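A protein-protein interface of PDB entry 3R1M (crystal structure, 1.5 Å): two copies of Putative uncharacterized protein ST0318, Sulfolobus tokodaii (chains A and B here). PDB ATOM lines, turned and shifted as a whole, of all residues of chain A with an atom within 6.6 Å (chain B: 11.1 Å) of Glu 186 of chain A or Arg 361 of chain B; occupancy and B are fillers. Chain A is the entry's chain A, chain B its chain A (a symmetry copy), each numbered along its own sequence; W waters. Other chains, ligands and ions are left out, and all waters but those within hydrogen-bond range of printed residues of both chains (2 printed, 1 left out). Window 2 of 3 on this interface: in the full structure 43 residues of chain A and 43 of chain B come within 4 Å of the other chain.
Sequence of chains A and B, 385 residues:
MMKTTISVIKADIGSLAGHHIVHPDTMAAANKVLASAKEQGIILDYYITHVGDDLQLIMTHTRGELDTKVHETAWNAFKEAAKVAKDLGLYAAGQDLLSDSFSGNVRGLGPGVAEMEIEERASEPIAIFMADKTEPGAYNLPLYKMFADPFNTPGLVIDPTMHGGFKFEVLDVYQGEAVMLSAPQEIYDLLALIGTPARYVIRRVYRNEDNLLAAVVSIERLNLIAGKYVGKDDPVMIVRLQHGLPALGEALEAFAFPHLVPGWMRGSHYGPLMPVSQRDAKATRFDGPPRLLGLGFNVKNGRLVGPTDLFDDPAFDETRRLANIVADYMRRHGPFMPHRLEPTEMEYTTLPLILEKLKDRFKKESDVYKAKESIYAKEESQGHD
Of the 14 printed residues of chain A, 6 touch a printed residue of chain B.
Printed residues of chain A that touch a printed residue of chain B: Ala 178, Val 179, Met 180, Leu 181, Glu 186 and Leu 191.
Hydrophobic or aromatic side chains of chain A within 4 Å of the printed part of chain B: Val 179, Leu 181 and Leu 191.
Along chain A the printed residues that touch a printed residue of chain B span positions 178 to 191.
Along chain B the printed residues that touch a printed residue of chain A span positions 336 to 363.
Among the printed residues, Asp or Glu carboxylates within 4 Å of a Lys or Arg side-chain nitrogen of the other chain: Glu 186 of chain A with Arg 361 of chain B (2.7 Å).
The side-chain carboxylate (OE2) of Glu 186 of chain A lies within salt-bridge range of the guanidinium group (NH1) of Arg 361 of chain B.
O of Ala 178 of chain A is in hydrogen-bond range of N of Lys 363 of chain B (2.9 Å).
NH2 of Arg 361 of chain B sits at hydrogen-bond distance from O of Met 180 of chain A (2.8 Å).
Of the printed residues of chain B, Met 180 of chain A touches Arg 361 (2.8 Å).
Leu 181 of chain A touches just one residue of chain B: Arg 361.
No residue of chain B comes within 4 Å of Ala 183 of chain A.
No residue of chain B comes within 4 Å of Pro 184 of chain A.
Of chain B, only Arg 361 (2.7 Å) comes within 4 Å of Glu 186 of chain A.
No residue of chain B comes within 4 Å of Ile 187 of chain A.
Tyr 188 of chain A touches none of the printed residues of chain B.
No residue of chain B comes within 4 Å of Asp 189 of chain A.
Of the printed residues of chain B, Leu 191 of chain A touches Phe 336.
Pro 335 of chain B touches none of the printed residues of chain A.
Arg 361 of chain B touches just these residues of chain A: Val 179 (3.6 Å), Met 180 (2.8 Å), Leu 181 (3.6 Å) and Glu 186 (2.7 Å).
Of the printed residues of chain A, Phe 362 of chain B touches Ala 178 and Val 179.
Of the printed residues of chain A, Lys 363 of chain B touches Ala 178 (2.9 Å).
The nearest residue of chain B that does not touch Glu 186 of chain A is Phe 362 of chain B (10.4 Å).
The nearest printed residue of chain B that does not touch Ala 178 of chain A is Arg 361 of chain B (4.1 Å).
Water W1 lies within hydrogen-bond range of the backbone carbonyl oxygen (O) of Lys 363 of chain B (2.5 Å), the backbone carbonyl oxygen (O) of Lys 364 of chain B (2.9 Å) and the backbone NH (N) of Ala 178 of chain A (3.5 Å).
Water W2 bridges O of Pro 335 of chain B and O of Leu 191 of chain A.
No position is printed for both chains.
Of the 8 pairs that touch across the chains among the printed residues, none has its exchanged pair printed and touching as well.
The backbone NH (N) of Ser 182 of chain A is in hydrogen-bond range of the side-chain carboxylate (OE1) of Glu 186 of chain A, 2.9 Å away.
O of Ala 178 of chain A touches CA of Phe 362 of chain B, 3.5 Å away.
CB of Arg 361 of chain B touches CG2 of Val 179 of chain A (3.6 Å).
CG1 of Val 179 of chain A touches CZ of Phe 362 of chain B, at 3.5 Å.
NH2 of Arg 361 of chain B touches CD2 of Leu 181 of chain A (3.6 Å).
Phe 336 of chain B touches Leu 191 of chain A (CE2 to CD2, 3.6 Å).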
ATOM      1  N   ALA A 178       2.113   7.607 -24.746  1.00  0.00           N
ATOM      2  CA  ALA A 178       3.238   8.097 -23.962  1.00  0.00           C
ATOM      3  C   ALA A 178       4.413   8.499 -24.851  1.00  0.00           C
ATOM      4  O   ALA A 178       4.580   7.970 -25.958  1.00  0.00           O
ATOM      5  CB  ALA A 178       3.661   7.058 -22.929  1.00  0.00           C
ATOM      6  N   VAL A 179       5.235   9.425 -24.369  1.00  0.00           N
ATOM      7  CA  VAL A 179       6.433   9.875 -25.067  1.00  0.00           C
ATOM      8  C   VAL A 179       7.598   9.825 -24.077  1.00  0.00           C
ATOM      9  O   VAL A 179       7.380   9.976 -22.866  1.00  0.00           O
ATOM     10  CB  VAL A 179       6.243  11.299 -25.643  1.00  0.00           C
ATOM     11  CG1 VAL A 179       6.085  12.322 -24.513  1.00  0.00           C
ATOM     12  CG2 VAL A 179       7.408  11.689 -26.515  1.00  0.00           C
ATOM     13  N   MET A 180       8.805   9.567 -24.563  1.00  0.00           N
ATOM     14  CA  MET A 180      10.028   9.626 -23.753  1.00  0.00           C
ATOM     15  C   MET A 180      10.759  10.927 -24.029  1.00  0.00           C
ATOM     16  O   MET A 180      11.032  11.244 -25.189  1.00  0.00           O
ATOM     17  CB  MET A 180      10.980   8.458 -24.097  1.00  0.00           C
ATOM     18  CG  MET A 180      10.443   7.075 -23.848  1.00  0.00           C
ATOM     19  SD  MET A 180      10.045   6.777 -22.114  1.00  0.00           S
ATOM     20  CE  MET A 180      11.455   7.505 -21.349  1.00  0.00           C
ATOM     21  N   LEU A 181      11.077  11.713 -22.989  1.00  0.00           N
ATOM     22  CA  LEU A 181      11.827  12.951 -23.171  1.00  0.00           C
ATOM     23  C   LEU A 181      13.033  12.905 -22.244  1.00  0.00           C
ATOM     24  O   LEU A 181      12.902  12.539 -21.079  1.00  0.00           O
ATOM     25  CB  LEU A 181      10.945  14.164 -22.832  1.00  0.00           C
ATOM     26  CG  LEU A 181       9.785  14.327 -23.818  1.00  0.00           C
ATOM     27  CD1 LEU A 181       8.766  15.347 -23.296  1.00  0.00           C
ATOM     28  CD2 LEU A 181      10.306  14.735 -25.193  1.00  0.00           C
ATOM     29  N   SER A 182      14.194  13.287 -22.754  1.00  0.00           N
ATOM     30  CA  SER A 182      15.443  13.155 -22.021  1.00  0.00           C
ATOM     31  C   SER A 182      15.917  14.506 -21.506  1.00  0.00           C
ATOM     32  O   SER A 182      15.905  15.490 -22.252  1.00  0.00           O
ATOM     33  CB  SER A 182      16.521  12.577 -22.943  1.00  0.00           C
ATOM     34  OG  SER A 182      17.776  12.578 -22.303  1.00  0.00           O
ATOM     35  N   ALA A 183      16.346  14.553 -20.239  1.00  0.00           N
ATOM     36  CA  ALA A 183      16.968  15.750 -19.669  1.00  0.00           C
ATOM     37  C   ALA A 183      18.488  15.600 -19.738  1.00  0.00           C
ATOM     38  O   ALA A 183      19.004  14.475 -19.635  1.00  0.00           O
ATOM     39  CB  ALA A 183      16.516  15.925 -18.215  1.00  0.00           C
ATOM     40  N   PRO A 184      19.216  16.719 -19.887  1.00  0.00           N
ATOM     41  CA  PRO A 184      18.677  18.070 -19.902  1.00  0.00           C
ATOM     42  C   PRO A 184      18.278  18.576 -21.285  1.00  0.00           C
ATOM     43  O   PRO A 184      17.751  19.668 -21.393  1.00  0.00           O
ATOM     44  CB  PRO A 184      19.841  18.910 -19.374  1.00  0.00           C
ATOM     45  CG  PRO A 184      21.052  18.166 -19.844  1.00  0.00           C
ATOM     46  CD  PRO A 184      20.691  16.713 -19.773  1.00  0.00           C
ATOM     47  N   GLN A 185      18.533  17.801 -22.342  1.00  0.00           N
ATOM     48  CA  GLN A 185      18.343  18.337 -23.686  1.00  0.00           C
ATOM     49  C   GLN A 185      16.909  18.757 -23.979  1.00  0.00           C
ATOM     50  O   GLN A 185      16.690  19.767 -24.658  1.00  0.00           O
ATOM     51  CB  GLN A 185      18.786  17.320 -24.753  1.00  0.00           C
ATOM     52  CG  GLN A 185      20.179  16.741 -24.514  1.00  0.00           C
ATOM     53  CD  GLN A 185      20.151  15.377 -23.828  1.00  0.00           C
ATOM     54  OE1 GLN A 185      19.443  15.156 -22.846  1.00  0.00           O
ATOM     55  NE2 GLN A 185      20.937  14.444 -24.363  1.00  0.00           N
ATOM     56  N   GLU A 186      15.943  18.008 -23.461  1.00  0.00           N
ATOM     57  CA  GLU A 186      14.539  18.228 -23.813  1.00  0.00           C
ATOM     58  C   GLU A 186      13.702  18.810 -22.663  1.00  0.00           C
ATOM     59  O   GLU A 186      12.477  18.669 -22.644  1.00  0.00           O
ATOM     60  CB  GLU A 186      13.921  16.933 -24.306  1.00  0.00           C
ATOM     61  CG  GLU A 186      14.711  16.345 -25.509  1.00  0.00           C
ATOM     62  CD  GLU A 186      14.041  15.148 -26.137  1.00  0.00           C
ATOM     63  OE1 GLU A 186      13.922  14.109 -25.492  1.00  0.00           O
ATOM     64  OE2 GLU A 186      13.654  15.243 -27.333  1.00  0.00           O
ATOM     65  N   ILE A 187      14.372  19.454 -21.722  1.00  0.00           N
ATOM     66  CA  ILE A 187      13.609  19.963 -20.559  1.00  0.00           C
ATOM     67  C   ILE A 187      12.528  20.993 -20.909  1.00  0.00           C
ATOM     68  O   ILE A 187      11.487  21.018 -20.251  1.00  0.00           O
ATOM     69  CB  ILE A 187      14.501  20.527 -19.410  1.00  0.00           C
ATOM     70  CG1 ILE A 187      15.456  21.634 -19.882  1.00  0.00           C
ATOM     71  CG2 ILE A 187      15.243  19.387 -18.685  1.00  0.00           C
ATOM     72  CD1 ILE A 187      16.097  22.427 -18.707  1.00  0.00           C
ATOM     73  N   TYR A 188      12.752  21.839 -21.920  1.00  0.00           N
ATOM     74  CA  TYR A 188      11.737  22.862 -22.233  1.00  0.00           C
ATOM     75  C   TYR A 188      10.490  22.191 -22.819  1.00  0.00           C
ATOM     76  O   TYR A 188       9.364  22.552 -22.506  1.00  0.00           O
ATOM     77  CB  TYR A 188      12.288  23.970 -23.142  1.00  0.00           C
ATOM     78  CG  TYR A 188      13.532  24.668 -22.609  1.00  0.00           C
ATOM     79  CD1 TYR A 188      13.817  24.719 -21.240  1.00  0.00           C
ATOM     80  CD2 TYR A 188      14.421  25.312 -23.479  1.00  0.00           C
ATOM     81  CE1 TYR A 188      14.990  25.362 -20.774  1.00  0.00           C
ATOM     82  CE2 TYR A 188      15.578  25.934 -23.019  1.00  0.00           C
ATOM     83  CZ  TYR A 188      15.849  25.965 -21.662  1.00  0.00           C
ATOM     84  OH  TYR A 188      16.986  26.579 -21.181  1.00  0.00           O
ATOM     85  N   ASP A 189      10.692  21.159 -23.638  1.00  0.00           N
ATOM     86  CA  ASP A 189       9.570  20.382 -24.153  1.00  0.00           C
ATOM     87  C   ASP A 189       8.861  19.606 -23.037  1.00  0.00           C
ATOM     88  O   ASP A 189       7.637  19.531 -22.974  1.00  0.00           O
ATOM     89  CB  ASP A 189      10.082  19.383 -25.194  1.00  0.00           C
ATOM     90  CG  ASP A 189      10.456  20.058 -26.473  1.00  0.00           C
ATOM     91  OD1 ASP A 189       9.741  21.014 -26.844  1.00  0.00           O
ATOM     92  OD2 ASP A 189      11.442  19.630 -27.102  1.00  0.00           O
ATOM     93  N   LEU A 190       9.664  18.966 -22.184  1.00  0.00           N
ATOM     94  CA  LEU A 190       9.135  18.256 -21.027  1.00  0.00           C
ATOM     95  C   LEU A 190       8.188  19.154 -20.193  1.00  0.00           C
ATOM     96  O   LEU A 190       7.056  18.756 -19.908  1.00  0.00           O
ATOM     97  CB  LEU A 190      10.307  17.739 -20.181  1.00  0.00           C
ATOM     98  CG  LEU A 190       9.928  17.011 -18.881  1.00  0.00           C
ATOM     99  CD1 LEU A 190       9.074  15.782 -19.153  1.00  0.00           C
ATOM    100  CD2 LEU A 190      11.187  16.638 -18.117  1.00  0.00           C
ATOM    101  N   LEU A 191       8.666  20.342 -19.836  1.00  0.00           N
ATOM    102  CA  LEU A 191       7.892  21.254 -18.988  1.00  0.00           C
ATOM    103  C   LEU A 191       6.641  21.797 -19.687  1.00  0.00           C
ATOM    104  O   LEU A 191       5.618  22.025 -19.043  1.00  0.00           O
ATOM    105  CB  LEU A 191       8.804  22.384 -18.509  1.00  0.00           C
ATOM    106  CG  LEU A 191       9.876  21.922 -17.491  1.00  0.00           C
ATOM    107  CD1 LEU A 191      10.962  22.954 -17.339  1.00  0.00           C
ATOM    108  CD2 LEU A 191       9.226  21.597 -16.151  1.00  0.00           C
ATOM    109  N   PRO B 335       6.877  26.791 -14.310  1.00  0.00           N
ATOM    110  CA  PRO B 335       5.896  26.713 -15.392  1.00  0.00           C
ATOM    111  C   PRO B 335       4.801  25.683 -15.162  1.00  0.00           C
ATOM    112  O   PRO B 335       4.216  25.173 -16.117  1.00  0.00           O
ATOM    113  CB  PRO B 335       6.768  26.340 -16.596  1.00  0.00           C
ATOM    114  CG  PRO B 335       7.828  25.457 -16.005  1.00  0.00           C
ATOM    115  CD  PRO B 335       8.136  26.086 -14.628  1.00  0.00           C
ATOM    116  N   PHE B 336       4.490  25.378 -13.900  1.00  0.00           N
ATOM    117  CA  PHE B 336       3.428  24.437 -13.580  1.00  0.00           C
ATOM    118  C   PHE B 336       2.128  25.126 -13.176  1.00  0.00           C
ATOM    119  O   PHE B 336       2.146  26.116 -12.440  1.00  0.00           O
ATOM    120  CB  PHE B 336       3.863  23.535 -12.413  1.00  0.00           C
ATOM    121  CG  PHE B 336       4.902  22.526 -12.781  1.00  0.00           C
ATOM    122  CD1 PHE B 336       4.512  21.234 -13.077  1.00  0.00           C
ATOM    123  CD2 PHE B 336       6.237  22.872 -12.880  1.00  0.00           C
ATOM    124  CE1 PHE B 336       5.482  20.294 -13.435  1.00  0.00           C
ATOM    125  CE2 PHE B 336       7.220  21.919 -13.207  1.00  0.00           C
ATOM    126  CZ  PHE B 336       6.810  20.642 -13.499  1.00  0.00           C
ATOM    127  N   ARG B 361       5.953  12.420 -31.159  1.00  0.00           N
ATOM    128  CA  ARG B 361       6.653  11.187 -30.792  1.00  0.00           C
ATOM    129  C   ARG B 361       5.807  10.255 -29.923  1.00  0.00           C
ATOM    130  O   ARG B 361       6.255   9.176 -29.533  1.00  0.00           O
ATOM    131  CB  ARG B 361       7.981  11.502 -30.096  1.00  0.00           C
ATOM    132  CG  ARG B 361       9.173  11.542 -31.042  1.00  0.00           C
ATOM    133  CD  ARG B 361      10.230  12.511 -30.552  1.00  0.00           C
ATOM    134  NE  ARG B 361      10.793  12.125 -29.262  1.00  0.00           N
ATOM    135  CZ  ARG B 361      11.634  12.886 -28.567  1.00  0.00           C
ATOM    136  NH1 ARG B 361      11.996  14.067 -29.043  1.00  0.00           N
ATOM    137  NH2 ARG B 361      12.109  12.471 -27.402  1.00  0.00           N
ATOM    138  N   PHE B 362       4.582  10.677 -29.629  1.00  0.00           N
ATOM    139  CA  PHE B 362       3.685   9.881 -28.799  1.00  0.00           C
ATOM    140  C   PHE B 362       3.372   8.511 -29.398  1.00  0.00           C
ATOM    141  O   PHE B 362       3.050   8.393 -30.583  1.00  0.00           O
ATOM    142  CB  PHE B 362       2.405  10.658 -28.489  1.00  0.00           C
ATOM    143  CG  PHE B 362       2.570  11.667 -27.386  1.00  0.00           C
ATOM    144  CD1 PHE B 362       2.385  11.299 -26.063  1.00  0.00           C
ATOM    145  CD2 PHE B 362       2.926  12.977 -27.668  1.00  0.00           C
ATOM    146  CE1 PHE B 362       2.542  12.221 -25.039  1.00  0.00           C
ATOM    147  CE2 PHE B 362       3.083  13.902 -26.653  1.00  0.00           C
ATOM    148  CZ  PHE B 362       2.889  13.526 -25.338  1.00  0.00           C
ATOM    149  N   LYS B 363       3.474   7.481 -28.562  1.00  0.00           N
ATOM    150  CA  LYS B 363       3.176   6.117 -28.970  1.00  0.00           C
ATOM    151  C   LYS B 363       2.068   5.500 -28.121  1.00  0.00           C
ATOM    152  O   LYS B 363       2.069   5.613 -26.895  1.00  0.00           O
ATOM    153  CB  LYS B 363       4.437   5.255 -28.914  1.00  0.00           C
ATOM    154  CG  LYS B 363       5.448   5.616 -29.985  1.00  0.00           C
ATOM    155  CD  LYS B 363       6.756   4.871 -29.801  1.00  0.00           C
ATOM    156  CE  LYS B 363       7.733   5.239 -30.904  1.00  0.00           C
ATOM    157  NZ  LYS B 363       9.085   4.678 -30.646  1.00  0.00           N
ATOM    158  N   LYS B 364       1.121   4.846 -28.788  1.00  0.00           N
ATOM    159  CA  LYS B 364       0.017   4.174 -28.112  1.00  0.00           C
ATOM    160  C   LYS B 364       0.498   3.285 -26.974  1.00  0.00           C
ATOM    161  O   LYS B 364      -0.135   3.229 -25.915  1.00  0.00           O
ATOM    162  CB  LYS B 364      -0.780   3.348 -29.119  1.00  0.00           C
ATOM    163  CG  LYS B 364      -1.335   4.177 -30.254  1.00  0.00           C
ATOM    164  CD  LYS B 364      -2.335   5.191 -29.721  1.00  0.00           C
ATOM    165  CE  LYS B 364      -3.454   4.489 -28.959  1.00  0.00           C
ATOM    166  NZ  LYS B 364      -4.547   5.428 -28.568  1.00  0.00           N
HETATM  167  O   HOH W   1       2.418   4.135 -24.858  1.00  0.00           O
HETATM  168  O   HOH W   2       4.129  24.409 -18.794  1.00  0.00           O
